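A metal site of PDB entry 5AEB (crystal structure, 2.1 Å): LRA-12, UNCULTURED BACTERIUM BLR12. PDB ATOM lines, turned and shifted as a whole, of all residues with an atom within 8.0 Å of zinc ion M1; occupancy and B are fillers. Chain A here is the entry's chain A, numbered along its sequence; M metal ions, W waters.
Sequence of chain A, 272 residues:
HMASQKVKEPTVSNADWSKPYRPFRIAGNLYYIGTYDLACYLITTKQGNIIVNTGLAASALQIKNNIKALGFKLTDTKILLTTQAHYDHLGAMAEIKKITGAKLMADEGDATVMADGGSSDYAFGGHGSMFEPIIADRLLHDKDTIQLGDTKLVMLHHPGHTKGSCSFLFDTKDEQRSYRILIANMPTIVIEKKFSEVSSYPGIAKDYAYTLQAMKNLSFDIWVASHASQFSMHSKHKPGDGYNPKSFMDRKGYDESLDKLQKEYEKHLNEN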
ATOM      1  N   TRP A  17     -28.896 -35.283  25.736  1.00  0.00           N
ATOM      2  CA  TRP A  17     -27.507 -34.965  25.423  1.00  0.00           C
ATOM      3  C   TRP A  17     -26.663 -36.202  25.307  1.00  0.00           C
ATOM      4  O   TRP A  17     -25.799 -36.274  24.465  1.00  0.00           O
ATOM      5  CB  TRP A  17     -26.929 -33.981  26.430  1.00  0.00           C
ATOM      6  CG  TRP A  17     -27.406 -32.561  26.244  1.00  0.00           C
ATOM      7  CD1 TRP A  17     -28.501 -32.102  25.487  1.00  0.00           C
ATOM      8  CD2 TRP A  17     -26.822 -31.335  26.833  1.00  0.00           C
ATOM      9  NE1 TRP A  17     -28.592 -30.734  25.549  1.00  0.00           N
ATOM     10  CE2 TRP A  17     -27.654 -30.215  26.351  1.00  0.00           C
ATOM     11  CE3 TRP A  17     -25.772 -31.083  27.691  1.00  0.00           C
ATOM     12  CZ2 TRP A  17     -27.380 -28.897  26.718  1.00  0.00           C
ATOM     13  CZ3 TRP A  17     -25.502 -29.748  28.034  1.00  0.00           C
ATOM     14  CH2 TRP A  17     -26.301 -28.680  27.568  1.00  0.00           C
ATOM     15  N   ASP A  37     -29.538 -35.069  20.881  1.00  0.00           N
ATOM     16  CA  ASP A  37     -29.494 -33.580  20.807  1.00  0.00           C
ATOM     17  C   ASP A  37     -28.126 -32.906  20.524  1.00  0.00           C
ATOM     18  O   ASP A  37     -28.091 -31.795  20.028  1.00  0.00           O
ATOM     19  CB  ASP A  37     -30.138 -32.921  22.027  1.00  0.00           C
ATOM     20  CG  ASP A  37     -30.499 -31.435  21.781  1.00  0.00           C
ATOM     21  OD1 ASP A  37     -31.252 -31.111  20.821  1.00  0.00           O
ATOM     22  OD2 ASP A  37     -30.047 -30.575  22.540  1.00  0.00           O
ATOM     23  N   LEU A  38     -27.000 -33.546  20.854  1.00  0.00           N
ATOM     24  CA  LEU A  38     -25.693 -32.924  20.551  1.00  0.00           C
ATOM     25  C   LEU A  38     -25.236 -33.299  19.158  1.00  0.00           C
ATOM     26  O   LEU A  38     -24.901 -34.448  18.882  1.00  0.00           O
ATOM     27  CB  LEU A  38     -24.646 -33.219  21.639  1.00  0.00           C
ATOM     28  CG  LEU A  38     -25.168 -32.935  23.047  1.00  0.00           C
ATOM     29  CD1 LEU A  38     -24.103 -33.190  24.103  1.00  0.00           C
ATOM     30  CD2 LEU A  38     -25.657 -31.488  23.126  1.00  0.00           C
ATOM     31  N   ALA A  39     -25.252 -32.322  18.270  1.00  0.00           N
ATOM     32  CA  ALA A  39     -25.074 -32.579  16.837  1.00  0.00           C
ATOM     33  C   ALA A  39     -23.605 -32.638  16.503  1.00  0.00           C
ATOM     34  O   ALA A  39     -22.839 -31.720  16.807  1.00  0.00           O
ATOM     35  CB  ALA A  39     -25.771 -31.500  16.021  1.00  0.00           C
ATOM     36  N   ASN A  53     -17.609 -31.076  15.823  1.00  0.00           N
ATOM     37  CA  ASN A  53     -18.136 -31.290  17.182  1.00  0.00           C
ATOM     38  C   ASN A  53     -18.010 -32.683  17.749  1.00  0.00           C
ATOM     39  O   ASN A  53     -17.954 -33.645  17.017  1.00  0.00           O
ATOM     40  CB  ASN A  53     -19.601 -30.816  17.326  1.00  0.00           C
ATOM     41  CG  ASN A  53     -19.769 -29.335  17.017  1.00  0.00           C
ATOM     42  OD1 ASN A  53     -18.814 -28.526  17.158  1.00  0.00           O
ATOM     43  ND2 ASN A  53     -20.967 -28.961  16.599  1.00  0.00           N
ATOM     44  N   THR A  83     -18.033 -25.756  16.223  1.00  0.00           N
ATOM     45  CA  THR A  83     -18.751 -24.494  16.056  1.00  0.00           C
ATOM     46  C   THR A  83     -18.681 -23.566  17.298  1.00  0.00           C
ATOM     47  O   THR A  83     -19.183 -22.415  17.246  1.00  0.00           O
ATOM     48  CB  THR A  83     -20.204 -24.779  15.730  1.00  0.00           C
ATOM     49  OG1 THR A  83     -20.726 -25.677  16.723  1.00  0.00           O
ATOM     50  CG2 THR A  83     -20.283 -25.460  14.327  1.00  0.00           C
ATOM     51  N   GLN A  84     -18.065 -24.033  18.385  1.00  0.00           N
ATOM     52  CA  GLN A  84     -18.424 -23.500  19.679  1.00  0.00           C
ATOM     53  C   GLN A  84     -17.572 -24.137  20.770  1.00  0.00           C
ATOM     54  O   GLN A  84     -17.691 -25.352  20.986  1.00  0.00           O
ATOM     55  CB  GLN A  84     -19.877 -24.018  19.949  1.00  0.00           C
ATOM     56  CG  GLN A  84     -20.783 -23.022  20.530  1.00  0.00           C
ATOM     57  CD  GLN A  84     -21.970 -23.671  21.162  1.00  0.00           C
ATOM     58  OE1 GLN A  84     -21.958 -23.924  22.391  1.00  0.00           O
ATOM     59  NE2 GLN A  84     -23.052 -23.913  20.336  1.00  0.00           N
ATOM     60  N   HIS A  86     -17.787 -24.984  23.982  1.00  0.00           N
ATOM     61  CA  HIS A  86     -18.497 -25.325  25.204  1.00  0.00           C
ATOM     62  C   HIS A  86     -18.417 -26.803  25.363  1.00  0.00           C
ATOM     63  O   HIS A  86     -18.340 -27.522  24.383  1.00  0.00           O
ATOM     64  CB  HIS A  86     -19.978 -24.937  25.136  1.00  0.00           C
ATOM     65  CG  HIS A  86     -20.261 -23.491  25.480  1.00  0.00           C
ATOM     66  ND1 HIS A  86     -21.401 -22.861  25.095  1.00  0.00           N
ATOM     67  CD2 HIS A  86     -19.503 -22.547  26.175  1.00  0.00           C
ATOM     68  CE1 HIS A  86     -21.360 -21.585  25.530  1.00  0.00           C
ATOM     69  NE2 HIS A  86     -20.202 -21.402  26.207  1.00  0.00           N
ATOM     70  N   TYR A  87     -18.518 -27.250  26.618  1.00  0.00           N
ATOM     71  CA  TYR A  87     -18.322 -28.655  26.976  1.00  0.00           C
ATOM     72  C   TYR A  87     -19.303 -29.605  26.294  1.00  0.00           C
ATOM     73  O   TYR A  87     -18.965 -30.775  26.105  1.00  0.00           O
ATOM     74  CB  TYR A  87     -18.374 -28.867  28.496  1.00  0.00           C
ATOM     75  CG  TYR A  87     -19.762 -28.778  29.099  1.00  0.00           C
ATOM     76  CD1 TYR A  87     -20.318 -27.553  29.451  1.00  0.00           C
ATOM     77  CD2 TYR A  87     -20.529 -29.933  29.286  1.00  0.00           C
ATOM     78  CE1 TYR A  87     -21.603 -27.463  29.999  1.00  0.00           C
ATOM     79  CE2 TYR A  87     -21.810 -29.859  29.827  1.00  0.00           C
ATOM     80  CZ  TYR A  87     -22.346 -28.638  30.185  1.00  0.00           C
ATOM     81  OH  TYR A  87     -23.633 -28.571  30.724  1.00  0.00           O
ATOM     82  N   ASP A  88     -20.491 -29.118  25.947  1.00  0.00           N
ATOM     83  CA  ASP A  88     -21.484 -29.930  25.232  1.00  0.00           C
ATOM     84  C   ASP A  88     -21.117 -30.178  23.746  1.00  0.00           C
ATOM     85  O   ASP A  88     -21.725 -31.027  23.099  1.00  0.00           O
ATOM     86  CB  ASP A  88     -22.967 -29.408  25.417  1.00  0.00           C
ATOM     87  CG  ASP A  88     -23.160 -27.949  24.990  1.00  0.00           C
ATOM     88  OD1 ASP A  88     -22.246 -27.107  25.271  1.00  0.00           O
ATOM     89  OD2 ASP A  88     -24.240 -27.639  24.372  1.00  0.00           O
ATOM     90  N   HIS A  89     -20.108 -29.476  23.236  1.00  0.00           N
ATOM     91  CA  HIS A  89     -19.620 -29.686  21.861  1.00  0.00           C
ATOM     92  C   HIS A  89     -18.162 -30.005  21.747  1.00  0.00           C
ATOM     93  O   HIS A  89     -17.680 -30.268  20.628  1.00  0.00           O
ATOM     94  CB  HIS A  89     -19.979 -28.496  20.986  1.00  0.00           C
ATOM     95  CG  HIS A  89     -21.394 -28.028  21.196  1.00  0.00           C
ATOM     96  ND1 HIS A  89     -22.429 -28.628  20.619  1.00  0.00           N
ATOM     97  CD2 HIS A  89     -21.918 -27.013  22.003  1.00  0.00           C
ATOM     98  CE1 HIS A  89     -23.571 -28.017  21.010  1.00  0.00           C
ATOM     99  NE2 HIS A  89     -23.248 -27.039  21.864  1.00  0.00           N
ATOM    100  N   HIS A 161     -22.260 -16.241  21.219  1.00  0.00           N
ATOM    101  CA  HIS A 161     -22.463 -17.472  22.010  1.00  0.00           C
ATOM    102  C   HIS A 161     -21.164 -17.818  22.713  1.00  0.00           C
ATOM    103  O   HIS A 161     -21.169 -18.082  23.928  1.00  0.00           O
ATOM    104  CB  HIS A 161     -22.932 -18.641  21.172  1.00  0.00           C
ATOM    105  CG  HIS A 161     -23.303 -19.884  21.992  1.00  0.00           C
ATOM    106  ND1 HIS A 161     -24.494 -20.022  22.585  1.00  0.00           N
ATOM    107  CD2 HIS A 161     -22.564 -21.023  22.325  1.00  0.00           C
ATOM    108  CE1 HIS A 161     -24.535 -21.191  23.254  1.00  0.00           C
ATOM    109  NE2 HIS A 161     -23.352 -21.813  23.085  1.00  0.00           N
ATOM    110  N   ASN A 185     -23.813 -22.130  13.826  1.00  0.00           N
ATOM    111  CA  ASN A 185     -23.931 -21.981  15.258  1.00  0.00           C
ATOM    112  C   ASN A 185     -24.946 -20.867  15.563  1.00  0.00           C
ATOM    113  O   ASN A 185     -24.655 -19.700  15.391  1.00  0.00           O
ATOM    114  CB  ASN A 185     -22.601 -21.704  15.928  1.00  0.00           C
ATOM    115  CG  ASN A 185     -22.694 -21.971  17.402  1.00  0.00           C
ATOM    116  OD1 ASN A 185     -22.846 -21.028  18.205  1.00  0.00           O
ATOM    117  ND2 ASN A 185     -22.736 -23.255  17.762  1.00  0.00           N
ATOM    118  N   THR A 188     -27.564 -18.062  20.273  1.00  0.00           N
ATOM    119  CA  THR A 188     -28.315 -18.092  21.483  1.00  0.00           C
ATOM    120  C   THR A 188     -27.500 -17.357  22.536  1.00  0.00           C
ATOM    121  O   THR A 188     -26.280 -17.227  22.412  1.00  0.00           O
ATOM    122  CB  THR A 188     -28.616 -19.548  21.880  1.00  0.00           C
ATOM    123  OG1 THR A 188     -27.369 -20.255  22.033  1.00  0.00           O
ATOM    124  CG2 THR A 188     -29.500 -20.251  20.794  1.00  0.00           C
ATOM    125  N   VAL A 190     -26.346 -17.100  26.473  1.00  0.00           N
ATOM    126  CA  VAL A 190     -26.057 -18.047  27.516  1.00  0.00           C
ATOM    127  C   VAL A 190     -26.196 -17.398  28.895  1.00  0.00           C
ATOM    128  O   VAL A 190     -26.469 -18.071  29.884  1.00  0.00           O
ATOM    129  CB  VAL A 190     -24.630 -18.649  27.275  1.00  0.00           C
ATOM    130  CG1 VAL A 190     -23.976 -19.147  28.544  1.00  0.00           C
ATOM    131  CG2 VAL A 190     -24.704 -19.753  26.233  1.00  0.00           C
ATOM    132  N   SER A 226     -25.878 -26.719  15.964  1.00  0.00           N
ATOM    133  CA  SER A 226     -25.116 -27.397  16.994  1.00  0.00           C
ATOM    134  C   SER A 226     -25.971 -28.334  17.870  1.00  0.00           C
ATOM    135  O   SER A 226     -25.470 -29.305  18.409  1.00  0.00           O
ATOM    136  CB  SER A 226     -24.380 -26.371  17.850  1.00  0.00           C
ATOM    137  OG  SER A 226     -23.280 -25.823  17.093  1.00  0.00           O
ATOM    138  N   HIS A 227     -27.262 -28.031  18.001  1.00  0.00           N
ATOM    139  CA  HIS A 227     -28.203 -28.916  18.721  1.00  0.00           C
ATOM    140  C   HIS A 227     -29.272 -29.373  17.760  1.00  0.00           C
ATOM    141  O   HIS A 227     -29.781 -28.555  16.989  1.00  0.00           O
ATOM    142  CB  HIS A 227     -28.835 -28.188  19.914  1.00  0.00           C
ATOM    143  CG  HIS A 227     -27.886 -27.970  21.073  1.00  0.00           C
ATOM    144  ND1 HIS A 227     -27.891 -28.757  22.171  1.00  0.00           N
ATOM    145  CD2 HIS A 227     -26.902 -27.011  21.274  1.00  0.00           C
ATOM    146  CE1 HIS A 227     -26.893 -28.349  23.004  1.00  0.00           C
ATOM    147  NE2 HIS A 227     -26.308 -27.268  22.474  1.00  0.00           N
ATOM    148  N   GLN A 230     -32.390 -27.311  17.616  1.00  0.00           N
ATOM    149  CA  GLN A 230     -32.362 -25.959  17.013  1.00  0.00           C
ATOM    150  C   GLN A 230     -32.718 -25.903  15.539  1.00  0.00           C
ATOM    151  O   GLN A 230     -33.134 -24.876  15.068  1.00  0.00           O
ATOM    152  CB  GLN A 230     -31.040 -25.239  17.265  1.00  0.00           C
ATOM    153  CG  GLN A 230     -30.719 -25.077  18.730  1.00  0.00           C
ATOM    154  CD  GLN A 230     -29.261 -24.677  18.969  1.00  0.00           C
ATOM    155  OE1 GLN A 230     -28.317 -25.123  18.251  1.00  0.00           O
ATOM    156  NE2 GLN A 230     -29.060 -23.829  19.944  1.00  0.00           N
HETATM  157 ZN    ZN M   1     -24.616 -26.285  23.010  1.00  0.00          ZN
HETATM  158 ZN    ZN M   2     -22.802 -23.295  23.863  1.00  0.00          ZN
HETATM  159  O   HOH W   1     -23.712 -24.934  24.036  1.00  0.00           O
HETATM  160  O   HOH W   2     -25.352 -24.629  22.492  1.00  0.00           O
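NE2 of His 89 lies close to NE2 of Gln 84 (3.5 Å).
N of His 227 is in hydrogen-bond range of OE1 of Gln 230.
A ring nitrogen (ND1) of His 227 is in hydrogen-bond range of the side-chain carboxylate of Asp 37, 2.8 Å away.
The side-chain amide nitrogen (NE2) of Gln 84 lies close to the side-chain amide nitrogen (ND2) of Asn 185, 2.7 Å away.
Gln 84 touches zinc ion M1 (OE1 to ZN, 3.6 Å).
Four residues have an atom within 4 Å of zinc ion M1: Gln 84, Asp 88, His 89 and His 227.
The nearest printed residue that does not touch zinc ion M1 is His 161 (4.6 Å).
Zinc ion M1 is bound by water W2 (1.9 Å), water W1 (1.9 Å), NE2 of His 89 (1.9 Å), OD2 of Asp 88 (2.0 Å) and NE2 of His 227 (2.0 Å).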
